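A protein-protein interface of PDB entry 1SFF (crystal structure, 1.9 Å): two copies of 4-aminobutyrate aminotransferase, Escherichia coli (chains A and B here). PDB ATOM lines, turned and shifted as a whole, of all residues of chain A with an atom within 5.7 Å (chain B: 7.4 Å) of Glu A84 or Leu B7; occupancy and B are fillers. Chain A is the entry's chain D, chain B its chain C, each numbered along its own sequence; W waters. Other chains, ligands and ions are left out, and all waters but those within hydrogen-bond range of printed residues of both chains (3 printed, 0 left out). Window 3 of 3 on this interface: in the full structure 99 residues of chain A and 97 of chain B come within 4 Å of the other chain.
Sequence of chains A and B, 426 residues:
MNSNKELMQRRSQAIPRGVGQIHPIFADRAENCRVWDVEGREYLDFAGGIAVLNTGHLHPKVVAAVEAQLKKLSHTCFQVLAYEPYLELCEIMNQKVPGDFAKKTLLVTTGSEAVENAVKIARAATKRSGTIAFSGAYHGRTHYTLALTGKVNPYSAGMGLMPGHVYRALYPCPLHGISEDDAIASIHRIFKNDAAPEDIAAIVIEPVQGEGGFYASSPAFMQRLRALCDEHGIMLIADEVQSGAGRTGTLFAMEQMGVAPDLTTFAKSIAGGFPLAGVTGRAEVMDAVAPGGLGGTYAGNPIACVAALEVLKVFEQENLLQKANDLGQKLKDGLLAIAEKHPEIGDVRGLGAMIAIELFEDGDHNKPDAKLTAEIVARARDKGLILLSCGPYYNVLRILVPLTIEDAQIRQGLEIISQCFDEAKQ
Ala A82 touches Phe B26 (O to CA, 3.4 Å). CD2 of Phe B26 touches C of Tyr A83 (3.5 Å). Ala B27 touches Tyr A83. CD2 of Leu B7 touches OE2 of Glu A84 (3.9 Å). Glu A84 touches Phe B26. OE1 of Glu A84 touches CG1 of Val B38 (3.8 Å). Tyr A86 touches Ile B15 (CE2 to CD1, 3.7 Å). Leu A87 touches Leu B7. Leu A87 touches Arg B10 (CD2 to NE, 3.7 Å). Arg B11 touches Leu A87 (CA to CD1, 3.7 Å).
OD1 of Asn B4 is in hydrogen-bond range of N of Phe B26 (2.9 Å). N of Val B38 sits at hydrogen-bond distance from O of Phe B26 (3.0 Å).
No position is printed for both chains. Of the 14 pairs that touch across the chains among the printed residues, none has its exchanged pair printed and touching as well.
Glu A84 touches just these residues of chain B: Leu B7, Phe B26 and Val B38. Of chain A, only Glu A84 and Leu A87 come within 4 Å of Leu B7. Printed residues of chain B within 4 Å of Lys A72: Asp B28 (2.7 Å). Of the printed residues of chain B, Leu A87 touches Leu B7, Arg B10, Arg B11 and Phe B26. Pro A85 touches none of the printed residues of chain B. Pro B24 touches none of the printed residues of chain A. The nearest printed residue of chain B that does not touch Glu A84 is Asp B28 (4.7 Å). The nearest printed residue of chain A that does not touch Leu B7 is Tyr A83 (6.4 Å). The nearest printed residue of chain A that does not touch Phe B26 is Pro A85 (6.4 Å).
Hydrophobic or aromatic side chains of chain B within 4 Å of the printed part of chain A: Leu B7, Ile B15, Phe B26, Ala B27 and Val B38. Of the 10 printed residues of chain A, 6 touch a printed residue of chain B. Hydrophobic or aromatic side chains of chain A within 4 Å of the printed part of chain B: Ala A82, Tyr A83, Tyr A86 and Leu A87. Among the printed residues, 14 pairs touch across the chains. Among the printed residues, Asp or Glu carboxylates within 4 Å of a Lys or Arg side-chain nitrogen of the other chain: Lys A72 with Asp B28 (2.7 Å).
Water W2 bridges OE1 of Glu A84 (2.4 Å) and OD1 of Asp B28 (2.8 Å). Water W1 bridges OE2 of Glu A84 (2.6 Å) and NH1 of Arg B10 (3.0 Å). Water W3 bridges the backbone carbonyl oxygen of Ala B27 and the backbone NH of Glu A84.
The backbone carbonyl oxygen of Ile B25 is in hydrogen-bond range of the backbone NH of Ala A82 (2.9 Å). NZ of Lys A72 lies within salt-bridge range of OD1 of Asp B28. The backbone carbonyl oxygen (O) of Ala A82 is in hydrogen-bond range of the backbone NH (N) of Ala B27 (2.8 Å).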
ATOM      1  N   LYS A  72      17.830 -23.864   4.410  1.00  0.00           N
ATOM      2  CA  LYS A  72      18.490 -24.980   5.125  1.00  0.00           C
ATOM      3  C   LYS A  72      17.737 -25.507   6.348  1.00  0.00           C
ATOM      4  O   LYS A  72      17.292 -26.673   6.376  1.00  0.00           O
ATOM      5  CB  LYS A  72      19.907 -24.535   5.512  1.00  0.00           C
ATOM      6  CG  LYS A  72      20.753 -24.165   4.245  1.00  0.00           C
ATOM      7  CD  LYS A  72      22.215 -23.788   4.537  1.00  0.00           C
ATOM      8  CE  LYS A  72      23.059 -25.008   4.941  1.00  0.00           C
ATOM      9  NZ  LYS A  72      24.560 -24.750   4.898  1.00  0.00           N
ATOM     10  N   ALA A  82      23.772 -29.456  17.129  1.00  0.00           N
ATOM     11  CA  ALA A  82      24.455 -28.177  16.910  1.00  0.00           C
ATOM     12  C   ALA A  82      24.343 -27.715  15.445  1.00  0.00           C
ATOM     13  O   ALA A  82      23.752 -28.414  14.614  1.00  0.00           O
ATOM     14  CB  ALA A  82      25.944 -28.305  17.312  1.00  0.00           C
ATOM     15  N   TYR A  83      24.865 -26.521  15.149  1.00  0.00           N
ATOM     16  CA  TYR A  83      24.893 -25.992  13.779  1.00  0.00           C
ATOM     17  C   TYR A  83      25.961 -24.943  13.725  1.00  0.00           C
ATOM     18  O   TYR A  83      26.232 -24.276  14.721  1.00  0.00           O
ATOM     19  CB  TYR A  83      23.525 -25.454  13.303  1.00  0.00           C
ATOM     20  CG  TYR A  83      22.735 -24.746  14.357  1.00  0.00           C
ATOM     21  CD1 TYR A  83      22.884 -23.361  14.573  1.00  0.00           C
ATOM     22  CD2 TYR A  83      21.859 -25.443  15.162  1.00  0.00           C
ATOM     23  CE1 TYR A  83      22.160 -22.703  15.593  1.00  0.00           C
ATOM     24  CE2 TYR A  83      21.124 -24.779  16.180  1.00  0.00           C
ATOM     25  CZ  TYR A  83      21.296 -23.425  16.382  1.00  0.00           C
ATOM     26  OH  TYR A  83      20.635 -22.789  17.429  1.00  0.00           O
ATOM     27  N   GLU A  84      26.587 -24.793  12.558  1.00  0.00           N
ATOM     28  CA  GLU A  84      27.716 -23.888  12.413  1.00  0.00           C
ATOM     29  C   GLU A  84      27.578 -22.392  12.682  1.00  0.00           C
ATOM     30  O   GLU A  84      28.502 -21.769  13.209  1.00  0.00           O
ATOM     31  CB  GLU A  84      28.318 -24.063  11.002  1.00  0.00           C
ATOM     32  CG  GLU A  84      28.966 -25.404  10.799  1.00  0.00           C
ATOM     33  CD  GLU A  84      29.572 -25.561   9.413  1.00  0.00           C
ATOM     34  OE1 GLU A  84      28.819 -25.812   8.446  1.00  0.00           O
ATOM     35  OE2 GLU A  84      30.798 -25.410   9.297  1.00  0.00           O
ATOM     36  N   PRO A  85      26.443 -21.779  12.274  1.00  0.00           N
ATOM     37  CA  PRO A  85      26.287 -20.340  12.506  1.00  0.00           C
ATOM     38  C   PRO A  85      26.437 -19.943  13.975  1.00  0.00           C
ATOM     39  O   PRO A  85      27.007 -18.904  14.264  1.00  0.00           O
ATOM     40  CB  PRO A  85      24.868 -20.051  11.964  1.00  0.00           C
ATOM     41  CG  PRO A  85      24.744 -21.033  10.833  1.00  0.00           C
ATOM     42  CD  PRO A  85      25.332 -22.310  11.460  1.00  0.00           C
ATOM     43  N   TYR A  86      25.911 -20.759  14.878  1.00  0.00           N
ATOM     44  CA  TYR A  86      26.000 -20.491  16.318  1.00  0.00           C
ATOM     45  C   TYR A  86      27.519 -20.541  16.691  1.00  0.00           C
ATOM     46  O   TYR A  86      28.076 -19.613  17.292  1.00  0.00           O
ATOM     47  CB  TYR A  86      25.182 -21.571  17.062  1.00  0.00           C
ATOM     48  CG  TYR A  86      25.058 -21.454  18.584  1.00  0.00           C
ATOM     49  CD1 TYR A  86      23.809 -21.506  19.214  1.00  0.00           C
ATOM     50  CD2 TYR A  86      26.184 -21.341  19.400  1.00  0.00           C
ATOM     51  CE1 TYR A  86      23.689 -21.456  20.611  1.00  0.00           C
ATOM     52  CE2 TYR A  86      26.067 -21.279  20.807  1.00  0.00           C
ATOM     53  CZ  TYR A  86      24.813 -21.334  21.398  1.00  0.00           C
ATOM     54  OH  TYR A  86      24.703 -21.220  22.775  1.00  0.00           O
ATOM     55  N   LEU A  87      28.195 -21.615  16.298  1.00  0.00           N
ATOM     56  CA  LEU A  87      29.626 -21.748  16.605  1.00  0.00           C
ATOM     57  C   LEU A  87      30.443 -20.603  16.051  1.00  0.00           C
ATOM     58  O   LEU A  87      31.257 -19.970  16.755  1.00  0.00           O
ATOM     59  CB  LEU A  87      30.157 -23.091  16.037  1.00  0.00           C
ATOM     60  CG  LEU A  87      31.673 -23.297  16.050  1.00  0.00           C
ATOM     61  CD1 LEU A  87      32.131 -23.310  17.533  1.00  0.00           C
ATOM     62  CD2 LEU A  87      32.036 -24.671  15.325  1.00  0.00           C
ATOM     63  N   GLU A  88      30.218 -20.298  14.773  1.00  0.00           N
ATOM     64  CA  GLU A  88      30.976 -19.263  14.138  1.00  0.00           C
ATOM     65  C   GLU A  88      30.763 -17.896  14.785  1.00  0.00           C
ATOM     66  O   GLU A  88      31.691 -17.118  14.927  1.00  0.00           O
ATOM     67  CB  GLU A  88      30.652 -19.245  12.632  1.00  0.00           C
ATOM     68  CG  GLU A  88      31.504 -18.239  11.863  1.00  0.00           C
ATOM     69  CD  GLU A  88      31.168 -18.236  10.376  1.00  0.00           C
ATOM     70  OE1 GLU A  88      31.661 -17.320   9.678  1.00  0.00           O
ATOM     71  OE2 GLU A  88      30.413 -19.165   9.944  1.00  0.00           O
ATOM     72  N   LEU A  89      29.538 -17.595  15.182  1.00  0.00           N
ATOM     73  CA  LEU A  89      29.278 -16.315  15.832  1.00  0.00           C
ATOM     74  C   LEU A  89      30.015 -16.255  17.202  1.00  0.00           C
ATOM     75  O   LEU A  89      30.607 -15.243  17.567  1.00  0.00           O
ATOM     76  CB  LEU A  89      27.767 -16.159  16.058  1.00  0.00           C
ATOM     77  CG  LEU A  89      27.088 -14.784  16.014  1.00  0.00           C
ATOM     78  CD1 LEU A  89      25.958 -14.718  17.036  1.00  0.00           C
ATOM     79  CD2 LEU A  89      28.080 -13.659  16.103  1.00  0.00           C
ATOM     80  N   LEU A 309      26.133 -12.644  11.944  1.00  0.00           N
ATOM     81  CA  LEU A 309      27.431 -12.795  11.250  1.00  0.00           C
ATOM     82  C   LEU A 309      27.473 -11.778  10.111  1.00  0.00           C
ATOM     83  O   LEU A 309      28.503 -11.155   9.853  1.00  0.00           O
ATOM     84  CB  LEU A 309      27.537 -14.214  10.674  1.00  0.00           C
ATOM     85  CG  LEU A 309      27.707 -15.264  11.777  1.00  0.00           C
ATOM     86  CD1 LEU A 309      27.509 -16.726  11.205  1.00  0.00           C
ATOM     87  CD2 LEU A 309      29.113 -15.098  12.431  1.00  0.00           C
ATOM     88  N   ASN B   2      34.643 -29.179   8.882  1.00  0.00           N
ATOM     89  CA  ASN B   2      33.534 -29.808   8.094  1.00  0.00           C
ATOM     90  C   ASN B   2      33.173 -31.233   8.530  1.00  0.00           C
ATOM     91  O   ASN B   2      32.364 -31.898   7.878  1.00  0.00           O
ATOM     92  CB  ASN B   2      33.838 -29.790   6.589  1.00  0.00           C
ATOM     93  CG  ASN B   2      35.082 -30.589   6.222  1.00  0.00           C
ATOM     94  OD1 ASN B   2      35.137 -31.823   6.384  1.00  0.00           O
ATOM     95  ND2 ASN B   2      36.094 -29.885   5.720  1.00  0.00           N
ATOM     96  N   SER B   3      33.796 -31.726   9.595  1.00  0.00           N
ATOM     97  CA  SER B   3      33.401 -33.024  10.126  1.00  0.00           C
ATOM     98  C   SER B   3      32.751 -32.676  11.473  1.00  0.00           C
ATOM     99  O   SER B   3      33.084 -31.629  12.082  1.00  0.00           O
ATOM    100  CB  SER B   3      34.605 -33.960  10.366  1.00  0.00           C
ATOM    101  OG  SER B   3      35.371 -33.590  11.510  1.00  0.00           O
ATOM    102  N   ASN B   4      31.830 -33.514  11.918  1.00  0.00           N
ATOM    103  CA  ASN B   4      31.195 -33.306  13.198  1.00  0.00           C
ATOM    104  C   ASN B   4      32.252 -33.228  14.295  1.00  0.00           C
ATOM    105  O   ASN B   4      32.143 -32.429  15.215  1.00  0.00           O
ATOM    106  CB  ASN B   4      30.291 -34.464  13.550  1.00  0.00           C
ATOM    107  CG  ASN B   4      29.010 -34.473  12.751  1.00  0.00           C
ATOM    108  OD1 ASN B   4      28.416 -33.428  12.510  1.00  0.00           O
ATOM    109  ND2 ASN B   4      28.565 -35.664  12.357  1.00  0.00           N
ATOM    110  N   LYS B   5      33.275 -34.077  14.220  1.00  0.00           N
ATOM    111  CA  LYS B   5      34.283 -34.087  15.276  1.00  0.00           C
ATOM    112  C   LYS B   5      35.084 -32.783  15.334  1.00  0.00           C
ATOM    113  O   LYS B   5      35.340 -32.271  16.418  1.00  0.00           O
ATOM    114  CB  LYS B   5      35.242 -35.273  15.099  1.00  0.00           C
ATOM    115  CG  LYS B   5      36.335 -35.348  16.159  1.00  0.00           C
ATOM    116  CD  LYS B   5      37.443 -36.351  15.715  1.00  0.00           C
ATOM    117  CE  LYS B   5      37.759 -37.462  16.765  1.00  0.00           C
ATOM    118  NZ  LYS B   5      38.403 -37.017  18.066  1.00  0.00           N
ATOM    119  N   GLU B   6      35.489 -32.251  14.185  1.00  0.00           N
ATOM    120  CA  GLU B   6      36.253 -31.001  14.178  1.00  0.00           C
ATOM    121  C   GLU B   6      35.383 -29.840  14.723  1.00  0.00           C
ATOM    122  O   GLU B   6      35.861 -28.943  15.432  1.00  0.00           O
ATOM    123  CB  GLU B   6      36.710 -30.670  12.758  1.00  0.00           C
ATOM    124  CG  GLU B   6      37.750 -31.638  12.222  1.00  0.00           C
ATOM    125  CD  GLU B   6      38.266 -31.252  10.829  1.00  0.00           C
ATOM    126  OE1 GLU B   6      37.434 -31.077   9.894  1.00  0.00           O
ATOM    127  OE2 GLU B   6      39.508 -31.129  10.687  1.00  0.00           O
ATOM    128  N   LEU B   7      34.106 -29.846  14.362  1.00  0.00           N
ATOM    129  CA  LEU B   7      33.220 -28.777  14.834  1.00  0.00           C
ATOM    130  C   LEU B   7      33.015 -28.931  16.344  1.00  0.00           C
ATOM    131  O   LEU B   7      32.898 -27.938  17.028  1.00  0.00           O
ATOM    132  CB  LEU B   7      31.890 -28.799  14.063  1.00  0.00           C
ATOM    133  CG  LEU B   7      32.066 -28.461  12.579  1.00  0.00           C
ATOM    134  CD1 LEU B   7      30.777 -28.735  11.821  1.00  0.00           C
ATOM    135  CD2 LEU B   7      32.471 -26.987  12.433  1.00  0.00           C
ATOM    136  N   MET B   8      32.964 -30.163  16.860  1.00  0.00           N
ATOM    137  CA  MET B   8      32.837 -30.344  18.301  1.00  0.00           C
ATOM    138  C   MET B   8      34.095 -29.853  19.021  1.00  0.00           C
ATOM    139  O   MET B   8      34.006 -29.341  20.136  1.00  0.00           O
ATOM    140  CB  MET B   8      32.586 -31.796  18.666  1.00  0.00           C
ATOM    141  CG  MET B   8      31.161 -32.264  18.330  1.00  0.00           C
ATOM    142  SD  MET B   8      29.873 -31.408  19.380  1.00  0.00           S
ATOM    143  CE  MET B   8      30.352 -31.931  21.018  1.00  0.00           C
ATOM    144  N   GLN B   9      35.270 -30.023  18.405  1.00  0.00           N
ATOM    145  CA  GLN B   9      36.516 -29.532  19.028  1.00  0.00           C
ATOM    146  C   GLN B   9      36.493 -28.008  19.059  1.00  0.00           C
ATOM    147  O   GLN B   9      36.835 -27.385  20.064  1.00  0.00           O
ATOM    148  CB  GLN B   9      37.742 -30.034  18.246  1.00  0.00           C
ATOM    149  CG  GLN B   9      37.870 -31.572  18.322  1.00  0.00           C
ATOM    150  CD  GLN B   9      38.974 -32.094  17.407  1.00  0.00           C
ATOM    151  OE1 GLN B   9      39.388 -31.405  16.482  1.00  0.00           O
ATOM    152  NE2 GLN B   9      39.432 -33.320  17.656  1.00  0.00           N
ATOM    153  N   ARG B  10      36.082 -27.397  17.958  1.00  0.00           N
ATOM    154  CA  ARG B  10      36.000 -25.933  17.942  1.00  0.00           C
ATOM    155  C   ARG B  10      34.978 -25.473  19.010  1.00  0.00           C
ATOM    156  O   ARG B  10      35.198 -24.481  19.701  1.00  0.00           O
ATOM    157  CB  ARG B  10      35.571 -25.422  16.558  1.00  0.00           C
ATOM    158  CG  ARG B  10      36.712 -25.292  15.572  1.00  0.00           C
ATOM    159  CD  ARG B  10      36.179 -25.152  14.138  1.00  0.00           C
ATOM    160  NE  ARG B  10      35.394 -23.920  13.978  1.00  0.00           N
ATOM    161  CZ  ARG B  10      34.717 -23.579  12.881  1.00  0.00           C
ATOM    162  NH1 ARG B  10      34.699 -24.370  11.819  1.00  0.00           N
ATOM    163  NH2 ARG B  10      34.080 -22.419  12.833  1.00  0.00           N
ATOM    164  N   ARG B  11      33.881 -26.204  19.125  1.00  0.00           N
ATOM    165  CA  ARG B  11      32.852 -25.884  20.132  1.00  0.00           C
ATOM    166  C   ARG B  11      33.457 -25.827  21.548  1.00  0.00           C
ATOM    167  O   ARG B  11      33.205 -24.878  22.297  1.00  0.00           O
ATOM    168  CB  ARG B  11      31.750 -26.953  20.105  1.00  0.00           C
ATOM    169  CG  ARG B  11      30.468 -26.648  20.962  1.00  0.00           C
ATOM    170  CD  ARG B  11      29.888 -27.960  21.470  1.00  0.00           C
ATOM    171  NE  ARG B  11      28.471 -27.902  21.907  1.00  0.00           N
ATOM    172  CZ  ARG B  11      28.049 -27.485  23.103  1.00  0.00           C
ATOM    173  NH1 ARG B  11      28.912 -27.057  24.041  1.00  0.00           N
ATOM    174  NH2 ARG B  11      26.744 -27.521  23.366  1.00  0.00           N
ATOM    175  N   SER B  12      34.303 -26.808  21.894  1.00  0.00           N
ATOM    176  CA  SER B  12      34.893 -26.867  23.229  1.00  0.00           C
ATOM    177  C   SER B  12      35.734 -25.646  23.525  1.00  0.00           C
ATOM    178  O   SER B  12      35.969 -25.318  24.679  1.00  0.00           O
ATOM    179  CB  SER B  12      35.784 -28.136  23.371  1.00  0.00           C
ATOM    180  OG  SER B  12      36.958 -27.968  22.578  1.00  0.00           O
ATOM    181  N   GLN B  13      36.214 -24.979  22.491  1.00  0.00           N
ATOM    182  CA  GLN B  13      37.057 -23.796  22.705  1.00  0.00           C
ATOM    183  C   GLN B  13      36.261 -22.482  22.672  1.00  0.00           C
ATOM    184  O   GLN B  13      36.706 -21.463  23.184  1.00  0.00           O
ATOM    185  CB  GLN B  13      38.164 -23.755  21.616  1.00  0.00           C
ATOM    186  CG  GLN B  13      39.123 -25.003  21.729  1.00  0.00           C
ATOM    187  CD  GLN B  13      39.599 -25.084  23.166  1.00  0.00           C
ATOM    188  OE1 GLN B  13      40.352 -24.209  23.623  1.00  0.00           O
ATOM    189  NE2 GLN B  13      39.122 -26.084  23.905  1.00  0.00           N
ATOM    190  N   ILE B  15      32.540 -22.187  23.193  1.00  0.00           N
ATOM    191  CA  ILE B  15      31.252 -22.206  23.898  1.00  0.00           C
ATOM    192  C   ILE B  15      31.362 -22.856  25.253  1.00  0.00           C
ATOM    193  O   ILE B  15      32.098 -23.844  25.421  1.00  0.00           O
ATOM    194  CB  ILE B  15      30.277 -22.964  22.994  1.00  0.00           C
ATOM    195  CG1 ILE B  15      30.094 -22.153  21.692  1.00  0.00           C
ATOM    196  CG2 ILE B  15      28.916 -23.239  23.674  1.00  0.00           C
ATOM    197  CD1 ILE B  15      29.311 -22.943  20.608  1.00  0.00           C
ATOM    198  N   PRO B  24      26.494 -35.173  19.473  1.00  0.00           N
ATOM    199  CA  PRO B  24      27.687 -34.482  18.973  1.00  0.00           C
ATOM    200  C   PRO B  24      27.728 -34.403  17.455  1.00  0.00           C
ATOM    201  O   PRO B  24      28.714 -34.785  16.795  1.00  0.00           O
ATOM    202  CB  PRO B  24      28.828 -35.306  19.561  1.00  0.00           C
ATOM    203  CG  PRO B  24      28.294 -36.716  19.439  1.00  0.00           C
ATOM    204  CD  PRO B  24      26.783 -36.585  19.805  1.00  0.00           C
ATOM    205  N   ILE B  25      26.650 -33.842  16.924  1.00  0.00           N
ATOM    206  CA  ILE B  25      26.417 -33.720  15.502  1.00  0.00           C
ATOM    207  C   ILE B  25      26.018 -32.298  15.132  1.00  0.00           C
ATOM    208  O   ILE B  25      25.235 -31.662  15.850  1.00  0.00           O
ATOM    209  CB  ILE B  25      25.257 -34.669  15.133  1.00  0.00           C
ATOM    210  CG1 ILE B  25      25.692 -36.128  15.360  1.00  0.00           C
ATOM    211  CG2 ILE B  25      24.816 -34.458  13.706  1.00  0.00           C
ATOM    212  CD1 ILE B  25      24.494 -37.079  15.482  1.00  0.00           C
ATOM    213  N   PHE B  26      26.568 -31.808  14.026  1.00  0.00           N
ATOM    214  CA  PHE B  26      26.239 -30.487  13.520  1.00  0.00           C
ATOM    215  C   PHE B  26      25.306 -30.658  12.321  1.00  0.00           C
ATOM    216  O   PHE B  26      25.686 -31.218  11.282  1.00  0.00           O
ATOM    217  CB  PHE B  26      27.508 -29.732  13.116  1.00  0.00           C
ATOM    218  CG  PHE B  26      28.158 -28.990  14.278  1.00  0.00           C
ATOM    219  CD1 PHE B  26      28.731 -29.694  15.339  1.00  0.00           C
ATOM    220  CD2 PHE B  26      28.162 -27.594  14.309  1.00  0.00           C
ATOM    221  CE1 PHE B  26      29.308 -29.029  16.429  1.00  0.00           C
ATOM    222  CE2 PHE B  26      28.736 -26.903  15.389  1.00  0.00           C
ATOM    223  CZ  PHE B  26      29.311 -27.620  16.452  1.00  0.00           C
ATOM    224  N   ALA B  27      24.063 -30.219  12.500  1.00  0.00           N
ATOM    225  CA  ALA B  27      23.049 -30.285  11.454  1.00  0.00           C
ATOM    226  C   ALA B  27      23.328 -29.219  10.413  1.00  0.00           C
ATOM    227  O   ALA B  27      23.747 -28.101  10.745  1.00  0.00           O
ATOM    228  CB  ALA B  27      21.647 -30.061  12.055  1.00  0.00           C
ATOM    229  N   ASP B  28      23.121 -29.561   9.141  1.00  0.00           N
ATOM    230  CA  ASP B  28      23.334 -28.591   8.076  1.00  0.00           C
ATOM    231  C   ASP B  28      21.990 -28.145   7.446  1.00  0.00           C
ATOM    232  O   ASP B  28      21.787 -26.969   7.165  1.00  0.00           O
ATOM    233  CB  ASP B  28      24.213 -29.185   6.976  1.00  0.00           C
ATOM    234  CG  ASP B  28      24.392 -28.242   5.792  1.00  0.00           C
ATOM    235  OD1 ASP B  28      25.141 -27.232   5.890  1.00  0.00           O
ATOM    236  OD2 ASP B  28      23.761 -28.493   4.755  1.00  0.00           O
ATOM    237  N   VAL B  38      26.664 -32.110   8.623  1.00  0.00           N
ATOM    238  CA  VAL B  38      27.669 -31.500   7.759  1.00  0.00           C
ATOM    239  C   VAL B  38      28.425 -32.559   6.956  1.00  0.00           C
ATOM    240  O   VAL B  38      29.142 -32.232   6.024  1.00  0.00           O
ATOM    241  CB  VAL B  38      28.685 -30.669   8.585  1.00  0.00           C
ATOM    242  CG1 VAL B  38      27.978 -29.456   9.235  1.00  0.00           C
ATOM    243  CG2 VAL B  38      29.295 -31.549   9.692  1.00  0.00           C
ATOM    244  N   GLU B  39      28.277 -33.812   7.338  1.00  0.00           N
ATOM    245  CA  GLU B  39      28.968 -34.889   6.632  1.00  0.00           C
ATOM    246  C   GLU B  39      28.028 -35.536   5.620  1.00  0.00           C
ATOM    247  O   GLU B  39      28.374 -36.523   4.963  1.00  0.00           O
ATOM    248  CB  GLU B  39      29.467 -35.919   7.635  1.00  0.00           C
ATOM    249  CG  GLU B  39      30.626 -35.392   8.496  1.00  0.00           C
ATOM    250  CD  GLU B  39      30.989 -36.325   9.642  1.00  0.00           C
ATOM    251  OE1 GLU B  39      30.712 -37.540   9.515  1.00  0.00           O
ATOM    252  OE2 GLU B  39      31.547 -35.851  10.667  1.00  0.00           O
HETATM  253  O   HOH W   1      32.259 -23.490  10.272  1.00  0.00           O
HETATM  254  O   HOH W   2      26.464 -26.087   8.014  1.00  0.00           O
HETATM  255  O   HOH W   3      25.905 -26.505  10.586  1.00  0.00           O
